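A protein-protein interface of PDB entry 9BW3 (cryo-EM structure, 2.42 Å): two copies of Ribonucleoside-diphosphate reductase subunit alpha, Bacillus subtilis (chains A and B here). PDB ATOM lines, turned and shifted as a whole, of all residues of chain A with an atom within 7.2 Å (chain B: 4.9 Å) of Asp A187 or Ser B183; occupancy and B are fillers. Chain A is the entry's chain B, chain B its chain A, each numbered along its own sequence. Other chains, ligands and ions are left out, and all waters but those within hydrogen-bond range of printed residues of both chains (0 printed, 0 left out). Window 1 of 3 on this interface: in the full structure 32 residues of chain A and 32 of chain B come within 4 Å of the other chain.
Of the 19 printed residues of chain A, 6 touch a printed residue of chain B.
Hydrophobic or aromatic side chains of chain A that line the printed part of chain B: Met A190.
Along chain A the printed residues that touch a printed residue of chain B span positions 183 to 447.
Of the 9 printed residues of chain B, 5 touch a printed residue of chain A.
Printed residues of chain B that touch a printed residue of chain A: Leu B179, Asn B180, Ser B183, Arg B184 and Asp B187.
Hydrophobic or aromatic side chains of chain B that line the printed part of chain A: Leu B179.
Among the printed residues, 8 pairs touch across the chains.
Ser A183 touches Asp B187, and with the chains exchanged Asp A187 touches Ser B183.
Arg B184 touches its own counterpart, Arg A184.
7 positions are printed for both chains.
Met A190 touches Leu B179 (O to CD2, 3.8 Å).
Ser B183 touches Met A190.
Leu B179 touches Gln A191.
Asp A181 touches none of the printed residues of chain B.
Asp A187 touches one residue of chain B.
Of the printed residues of chain B, Gln A191 touches Leu B179 and Asn B180.
Printed residues of chain B within 4 Å of Asn A447: Asn B180 (3.4 Å).
Of chain A, only Asp A187 (3.3 Å) and Met A190 (3.4 Å) come within 4 Å of Ser B183.
Of the printed residues of chain A, Arg B184 touches Arg A184 (2.9 Å).
The nearest residue of chain B that does not touch Asp A187 is Asn B180 (4.4 Å).
The nearest residue of chain A that does not touch Ser B183 is Gln A191 (4.6 Å).
The nearest printed residue of chain B that does not touch Asn A447 is Leu B179 (6.3 Å).
The side-chain amide oxygen (OD1) of Asn B180 sits at hydrogen-bond distance from the side-chain amide nitrogen (NE2) of Gln A191 (2.6 Å).
The side-chain amide oxygen of Asn B180 is in hydrogen-bond range of the side-chain amide nitrogen of Asn A447 (3.4 Å).
The side-chain hydroxyl of Ser B183 lies within hydrogen-bond range of the side-chain carboxylate of Asp A187.
The side-chain carboxylate of Asp B187 sits at hydrogen-bond distance from the side-chain hydroxyl of Ser A183.
The guanidinium group (NH2) of Arg A184 sits close to the guanidinium group (NH2) of Arg B184 (2.9 Å).
The backbone carbonyl oxygen (O) of Leu B179 lies within hydrogen-bond range of the side-chain hydroxyl (OG) of Ser B183 (3.4 Å).
NH1 of Arg B184 is in salt-bridge range of OD2 of Asp B187 (3.1 Å).
OD2 of Asp A187 is in salt-bridge range of NH1 of Arg A184 (3.3 Å).
NE2 of Gln A191 sits at hydrogen-bond distance from OD1 of Asp A187 (3.1 Å).
The side-chain amide oxygen (OE1) of Gln A191 is in hydrogen-bond range of the side-chain amide nitrogen (ND2) of Asn A447, 3.2 Å away.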
ATOM      1  N   LEU A 173      -1.850  22.062  11.182  1.00  0.00           N
ATOM      2  CA  LEU A 173      -1.461  20.820  10.532  1.00  0.00           C
ATOM      3  C   LEU A 173      -2.461  19.721  10.855  1.00  0.00           C
ATOM      4  O   LEU A 173      -2.738  19.452  12.027  1.00  0.00           O
ATOM      5  CB  LEU A 173      -0.059  20.386  10.968  1.00  0.00           C
ATOM      6  CG  LEU A 173       1.090  21.360  10.709  1.00  0.00           C
ATOM      7  CD1 LEU A 173       2.407  20.770  11.190  1.00  0.00           C
ATOM      8  CD2 LEU A 173       1.163  21.723   9.238  1.00  0.00           C
ATOM      9  N   ASP A 181       2.577   9.504   8.713  1.00  0.00           N
ATOM     10  CA  ASP A 181       1.949  10.802   8.921  1.00  0.00           C
ATOM     11  C   ASP A 181       2.422  11.451  10.216  1.00  0.00           C
ATOM     12  O   ASP A 181       2.636  12.663  10.259  1.00  0.00           O
ATOM     13  CB  ASP A 181       0.431  10.653   8.909  1.00  0.00           C
ATOM     14  CG  ASP A 181      -0.097  10.245   7.550  1.00  0.00           C
ATOM     15  OD1 ASP A 181       0.169  10.969   6.570  1.00  0.00           O
ATOM     16  OD2 ASP A 181      -0.769   9.198   7.460  1.00  0.00           O
ATOM     17  N   ILE A 182       2.596  10.665  11.280  1.00  0.00           N
ATOM     18  CA  ILE A 182       3.069  11.228  12.542  1.00  0.00           C
ATOM     19  C   ILE A 182       4.494  11.753  12.400  1.00  0.00           C
ATOM     20  O   ILE A 182       4.820  12.847  12.878  1.00  0.00           O
ATOM     21  CB  ILE A 182       2.959  10.181  13.666  1.00  0.00           C
ATOM     22  CG1 ILE A 182       1.502  10.017  14.102  1.00  0.00           C
ATOM     23  CG2 ILE A 182       3.827  10.573  14.848  1.00  0.00           C
ATOM     24  CD1 ILE A 182       1.229   8.731  14.844  1.00  0.00           C
ATOM     25  N   SER A 183       5.367  10.981  11.752  1.00  0.00           N
ATOM     26  CA  SER A 183       6.739  11.430  11.551  1.00  0.00           C
ATOM     27  C   SER A 183       6.787  12.673  10.671  1.00  0.00           C
ATOM     28  O   SER A 183       7.547  13.611  10.945  1.00  0.00           O
ATOM     29  CB  SER A 183       7.575  10.301  10.947  1.00  0.00           C
ATOM     30  OG  SER A 183       7.282  10.127   9.573  1.00  0.00           O
ATOM     31  N   ARG A 184       5.977  12.702   9.611  1.00  0.00           N
ATOM     32  CA  ARG A 184       5.915  13.889   8.767  1.00  0.00           C
ATOM     33  C   ARG A 184       5.379  15.085   9.538  1.00  0.00           C
ATOM     34  O   ARG A 184       5.822  16.216   9.324  1.00  0.00           O
ATOM     35  CB  ARG A 184       5.057  13.617   7.534  1.00  0.00           C
ATOM     36  CG  ARG A 184       5.126  14.719   6.498  1.00  0.00           C
ATOM     37  CD  ARG A 184       6.558  14.974   6.079  1.00  0.00           C
ATOM     38  NE  ARG A 184       7.077  13.903   5.238  1.00  0.00           N
ATOM     39  CZ  ARG A 184       8.210  13.970   4.554  1.00  0.00           C
ATOM     40  NH1 ARG A 184       8.984  15.042   4.603  1.00  0.00           N
ATOM     41  NH2 ARG A 184       8.576  12.935   3.804  1.00  0.00           N
ATOM     42  N   ALA A 185       4.411  14.862  10.427  1.00  0.00           N
ATOM     43  CA  ALA A 185       3.893  15.947  11.248  1.00  0.00           C
ATOM     44  C   ALA A 185       4.975  16.504  12.159  1.00  0.00           C
ATOM     45  O   ALA A 185       5.100  17.724  12.310  1.00  0.00           O
ATOM     46  CB  ALA A 185       2.699  15.464  12.068  1.00  0.00           C
ATOM     47  N   ILE A 186       5.767  15.627  12.774  1.00  0.00           N
ATOM     48  CA  ILE A 186       6.867  16.093  13.617  1.00  0.00           C
ATOM     49  C   ILE A 186       7.858  16.904  12.790  1.00  0.00           C
ATOM     50  O   ILE A 186       8.302  17.986  13.199  1.00  0.00           O
ATOM     51  CB  ILE A 186       7.555  14.904  14.312  1.00  0.00           C
ATOM     52  CG1 ILE A 186       6.616  14.256  15.329  1.00  0.00           C
ATOM     53  CG2 ILE A 186       8.844  15.353  14.983  1.00  0.00           C
ATOM     54  CD1 ILE A 186       7.020  12.854  15.719  1.00  0.00           C
ATOM     55  N   ASP A 187       8.210  16.395  11.608  1.00  0.00           N
ATOM     56  CA  ASP A 187       9.161  17.097  10.751  1.00  0.00           C
ATOM     57  C   ASP A 187       8.628  18.461  10.330  1.00  0.00           C
ATOM     58  O   ASP A 187       9.360  19.457  10.351  1.00  0.00           O
ATOM     59  CB  ASP A 187       9.485  16.244   9.525  1.00  0.00           C
ATOM     60  CG  ASP A 187      10.088  17.053   8.394  1.00  0.00           C
ATOM     61  OD1 ASP A 187      11.025  17.837   8.650  1.00  0.00           O
ATOM     62  OD2 ASP A 187       9.622  16.907   7.246  1.00  0.00           O
ATOM     63  N   ILE A 188       7.354  18.525   9.940  1.00  0.00           N
ATOM     64  CA  ILE A 188       6.760  19.782   9.498  1.00  0.00           C
ATOM     65  C   ILE A 188       6.668  20.766  10.654  1.00  0.00           C
ATOM     66  O   ILE A 188       6.908  21.965  10.483  1.00  0.00           O
ATOM     67  CB  ILE A 188       5.381  19.527   8.865  1.00  0.00           C
ATOM     68  CG1 ILE A 188       5.528  18.799   7.528  1.00  0.00           C
ATOM     69  CG2 ILE A 188       4.627  20.835   8.687  1.00  0.00           C
ATOM     70  CD1 ILE A 188       4.216  18.338   6.944  1.00  0.00           C
ATOM     71  N   SER A 189       6.298  20.285  11.841  1.00  0.00           N
ATOM     72  CA  SER A 189       6.246  21.160  13.005  1.00  0.00           C
ATOM     73  C   SER A 189       7.616  21.743  13.305  1.00  0.00           C
ATOM     74  O   SER A 189       7.740  22.937  13.601  1.00  0.00           O
ATOM     75  CB  SER A 189       5.713  20.394  14.215  1.00  0.00           C
ATOM     76  OG  SER A 189       4.389  19.947  13.995  1.00  0.00           O
ATOM     77  N   MET A 190       8.660  20.915  13.229  1.00  0.00           N
ATOM     78  CA  MET A 190      10.010  21.414  13.467  1.00  0.00           C
ATOM     79  C   MET A 190      10.423  22.420  12.399  1.00  0.00           C
ATOM     80  O   MET A 190      11.038  23.446  12.709  1.00  0.00           O
ATOM     81  CB  MET A 190      10.985  20.242  13.526  1.00  0.00           C
ATOM     82  CG  MET A 190      10.965  19.502  14.854  1.00  0.00           C
ATOM     83  SD  MET A 190      12.603  19.137  15.499  1.00  0.00           S
ATOM     84  CE  MET A 190      13.033  17.723  14.488  1.00  0.00           C
ATOM     85  N   GLN A 191      10.086  22.147  11.136  1.00  0.00           N
ATOM     86  CA  GLN A 191      10.422  23.071  10.058  1.00  0.00           C
ATOM     87  C   GLN A 191       9.718  24.410  10.233  1.00  0.00           C
ATOM     88  O   GLN A 191      10.305  25.468   9.977  1.00  0.00           O
ATOM     89  CB  GLN A 191      10.058  22.457   8.706  1.00  0.00           C
ATOM     90  CG  GLN A 191      10.773  21.158   8.382  1.00  0.00           C
ATOM     91  CD  GLN A 191      12.267  21.335   8.226  1.00  0.00           C
ATOM     92  OE1 GLN A 191      12.760  22.451   8.075  1.00  0.00           O
ATOM     93  NE2 GLN A 191      13.000  20.229   8.258  1.00  0.00           N
ATOM     94  N   LEU A 192       8.453  24.383  10.655  1.00  0.00           N
ATOM     95  CA  LEU A 192       7.678  25.611  10.794  1.00  0.00           C
ATOM     96  C   LEU A 192       8.088  26.397  12.032  1.00  0.00           C
ATOM     97  O   LEU A 192       8.109  27.632  12.003  1.00  0.00           O
ATOM     98  CB  LEU A 192       6.184  25.288  10.835  1.00  0.00           C
ATOM     99  CG  LEU A 192       5.587  24.668   9.571  1.00  0.00           C
ATOM    100  CD1 LEU A 192       4.158  24.218   9.817  1.00  0.00           C
ATOM    101  CD2 LEU A 192       5.655  25.638   8.405  1.00  0.00           C
ATOM    102  N   SER A 193       8.410  25.706  13.128  1.00  0.00           N
ATOM    103  CA  SER A 193       8.914  26.398  14.308  1.00  0.00           C
ATOM    104  C   SER A 193      10.300  26.971  14.058  1.00  0.00           C
ATOM    105  O   SER A 193      10.643  28.025  14.606  1.00  0.00           O
ATOM    106  CB  SER A 193       8.929  25.451  15.505  1.00  0.00           C
ATOM    107  OG  SER A 193       7.629  24.962  15.777  1.00  0.00           O
ATOM    108  N   LEU A 230       5.657  15.487  19.904  1.00  0.00           N
ATOM    109  CA  LEU A 230       5.522  16.855  19.416  1.00  0.00           C
ATOM    110  C   LEU A 230       6.095  17.861  20.403  1.00  0.00           C
ATOM    111  O   LEU A 230       6.695  18.861  19.997  1.00  0.00           O
ATOM    112  CB  LEU A 230       4.052  17.165  19.132  1.00  0.00           C
ATOM    113  CG  LEU A 230       3.440  16.473  17.915  1.00  0.00           C
ATOM    114  CD1 LEU A 230       1.931  16.649  17.908  1.00  0.00           C
ATOM    115  CD2 LEU A 230       4.056  17.007  16.634  1.00  0.00           C
ATOM    116  N   ALA A 233       9.727  17.786  19.994  1.00  0.00           N
ATOM    117  CA  ALA A 233      10.085  18.392  18.716  1.00  0.00           C
ATOM    118  C   ALA A 233      10.032  19.914  18.791  1.00  0.00           C
ATOM    119  O   ALA A 233      10.902  20.602  18.247  1.00  0.00           O
ATOM    120  CB  ALA A 233       9.163  17.875  17.613  1.00  0.00           C
ATOM    121  N   ASN A 447       8.968  23.123   2.892  1.00  0.00           N
ATOM    122  CA  ASN A 447       9.051  21.927   3.715  1.00  0.00           C
ATOM    123  C   ASN A 447       7.715  21.548   4.336  1.00  0.00           C
ATOM    124  O   ASN A 447       7.667  20.617   5.148  1.00  0.00           O
ATOM    125  CB  ASN A 447      10.099  22.112   4.819  1.00  0.00           C
ATOM    126  CG  ASN A 447      11.446  21.539   4.439  1.00  0.00           C
ATOM    127  OD1 ASN A 447      11.528  20.552   3.709  1.00  0.00           O
ATOM    128  ND2 ASN A 447      12.511  22.162   4.921  1.00  0.00           N
ATOM    129  N   ALA A 448       6.636  22.242   3.983  1.00  0.00           N
ATOM    130  CA  ALA A 448       5.284  21.920   4.437  1.00  0.00           C
ATOM    131  C   ALA A 448       4.392  21.874   3.204  1.00  0.00           C
ATOM    132  O   ALA A 448       3.718  22.858   2.874  1.00  0.00           O
ATOM    133  CB  ALA A 448       4.782  22.936   5.462  1.00  0.00           C
ATOM    134  N   PRO A 449       4.374  20.743   2.491  1.00  0.00           N
ATOM    135  CA  PRO A 449       3.650  20.709   1.208  1.00  0.00           C
ATOM    136  C   PRO A 449       2.183  21.071   1.333  1.00  0.00           C
ATOM    137  O   PRO A 449       1.654  21.791   0.477  1.00  0.00           O
ATOM    138  CB  PRO A 449       3.835  19.258   0.739  1.00  0.00           C
ATOM    139  CG  PRO A 449       4.946  18.711   1.561  1.00  0.00           C
ATOM    140  CD  PRO A 449       4.912  19.427   2.861  1.00  0.00           C
ATOM    141  N   LEU B 179      18.468  19.928   9.898  1.00  0.00           N
ATOM    142  CA  LEU B 179      17.150  19.626  10.447  1.00  0.00           C
ATOM    143  C   LEU B 179      16.420  18.598   9.595  1.00  0.00           C
ATOM    144  O   LEU B 179      15.748  17.707  10.125  1.00  0.00           O
ATOM    145  CB  LEU B 179      16.322  20.904  10.568  1.00  0.00           C
ATOM    146  CG  LEU B 179      14.948  20.736  11.223  1.00  0.00           C
ATOM    147  CD1 LEU B 179      15.092  20.394  12.698  1.00  0.00           C
ATOM    148  CD2 LEU B 179      14.102  21.984  11.035  1.00  0.00           C
ATOM    149  N   ASN B 180      16.530  18.710   8.270  1.00  0.00           N
ATOM    150  CA  ASN B 180      15.915  17.720   7.394  1.00  0.00           C
ATOM    151  C   ASN B 180      16.468  16.331   7.680  1.00  0.00           C
ATOM    152  O   ASN B 180      15.715  15.356   7.793  1.00  0.00           O
ATOM    153  CB  ASN B 180      16.150  18.096   5.932  1.00  0.00           C
ATOM    154  CG  ASN B 180      15.256  19.226   5.469  1.00  0.00           C
ATOM    155  OD1 ASN B 180      14.236  19.521   6.090  1.00  0.00           O
ATOM    156  ND2 ASN B 180      15.640  19.871   4.376  1.00  0.00           N
ATOM    157  N   ASP B 181      17.791  16.229   7.817  1.00  0.00           N
ATOM    158  CA  ASP B 181      18.414  14.940   8.081  1.00  0.00           C
ATOM    159  C   ASP B 181      18.050  14.417   9.465  1.00  0.00           C
ATOM    160  O   ASP B 181      17.859  13.212   9.642  1.00  0.00           O
ATOM    161  CB  ASP B 181      19.927  15.056   7.919  1.00  0.00           C
ATOM    162  CG  ASP B 181      20.344  15.193   6.467  1.00  0.00           C
ATOM    163  OD1 ASP B 181      20.092  14.254   5.686  1.00  0.00           O
ATOM    164  OD2 ASP B 181      20.920  16.240   6.107  1.00  0.00           O
ATOM    165  N   ILE B 182      17.939  15.302  10.457  1.00  0.00           N
ATOM    166  CA  ILE B 182      17.566  14.864  11.799  1.00  0.00           C
ATOM    167  C   ILE B 182      16.131  14.352  11.820  1.00  0.00           C
ATOM    168  O   ILE B 182      15.830  13.325  12.444  1.00  0.00           O
ATOM    169  CB  ILE B 182      17.778  16.006  12.809  1.00  0.00           C
ATOM    170  CG1 ILE B 182      19.261  16.138  13.156  1.00  0.00           C
ATOM    171  CG2 ILE B 182      16.947  15.772  14.062  1.00  0.00           C
ATOM    172  CD1 ILE B 182      19.623  17.460  13.784  1.00  0.00           C
ATOM    173  N   SER B 183      15.221  15.056  11.144  1.00  0.00           N
ATOM    174  CA  SER B 183      13.841  14.591  11.054  1.00  0.00           C
ATOM    175  C   SER B 183      13.759  13.258  10.325  1.00  0.00           C
ATOM    176  O   SER B 183      13.030  12.351  10.748  1.00  0.00           O
ATOM    177  CB  SER B 183      12.981  15.643  10.352  1.00  0.00           C
ATOM    178  OG  SER B 183      12.723  16.742  11.205  1.00  0.00           O
ATOM    179  N   ARG B 184      14.498  13.119   9.223  1.00  0.00           N
ATOM    180  CA  ARG B 184      14.508  11.851   8.504  1.00  0.00           C
ATOM    181  C   ARG B 184      15.079  10.735   9.369  1.00  0.00           C
ATOM    182  O   ARG B 184      14.606   9.597   9.315  1.00  0.00           O
ATOM    183  CB  ARG B 184      15.300  11.987   7.205  1.00  0.00           C
ATOM    184  CG  ARG B 184      15.226  10.761   6.320  1.00  0.00           C
ATOM    185  CD  ARG B 184      13.787  10.347   6.088  1.00  0.00           C
ATOM    186  NE  ARG B 184      13.074  11.311   5.262  1.00  0.00           N
ATOM    187  CZ  ARG B 184      11.879  11.101   4.727  1.00  0.00           C
ATOM    188  NH1 ARG B 184      11.214   9.977   4.939  1.00  0.00           N
ATOM    189  NH2 ARG B 184      11.338  12.042   3.960  1.00  0.00           N
ATOM    190  N   ALA B 185      16.104  11.040  10.164  1.00  0.00           N
ATOM    191  CA  ALA B 185      16.677  10.039  11.056  1.00  0.00           C
ATOM    192  C   ALA B 185      15.669   9.600  12.107  1.00  0.00           C
ATOM    193  O   ALA B 185      15.556   8.407  12.402  1.00  0.00           O
ATOM    194  CB  ALA B 185      17.939  10.586  11.719  1.00  0.00           C
ATOM    195  N   ILE B 186      14.935  10.550  12.687  1.00  0.00           N
ATOM    196  CA  ILE B 186      13.901  10.196  13.658  1.00  0.00           C
ATOM    197  C   ILE B 186      12.849   9.309  13.005  1.00  0.00           C
ATOM    198  O   ILE B 186      12.435   8.282  13.563  1.00  0.00           O
ATOM    199  CB  ILE B 186      13.272  11.466  14.259  1.00  0.00           C
ATOM    200  CG1 ILE B 186      14.247  12.149  15.218  1.00  0.00           C
ATOM    201  CG2 ILE B 186      11.970  11.133  14.972  1.00  0.00           C
ATOM    202  CD1 ILE B 186      13.906  13.594  15.499  1.00  0.00           C
ATOM    203  N   ASP B 187      12.409   9.688  11.804  1.00  0.00           N
ATOM    204  CA  ASP B 187      11.394   8.911  11.102  1.00  0.00           C
ATOM    205  C   ASP B 187      11.886   7.499  10.808  1.00  0.00           C
ATOM    206  O   ASP B 187      11.161   6.520  11.013  1.00  0.00           O
ATOM    207  CB  ASP B 187      10.993   9.621   9.810  1.00  0.00           C
ATOM    208  CG  ASP B 187      10.200   8.727   8.874  1.00  0.00           C
ATOM    209  OD1 ASP B 187       9.226   8.095   9.333  1.00  0.00           O
ATOM    210  OD2 ASP B 187      10.551   8.660   7.678  1.00  0.00           O
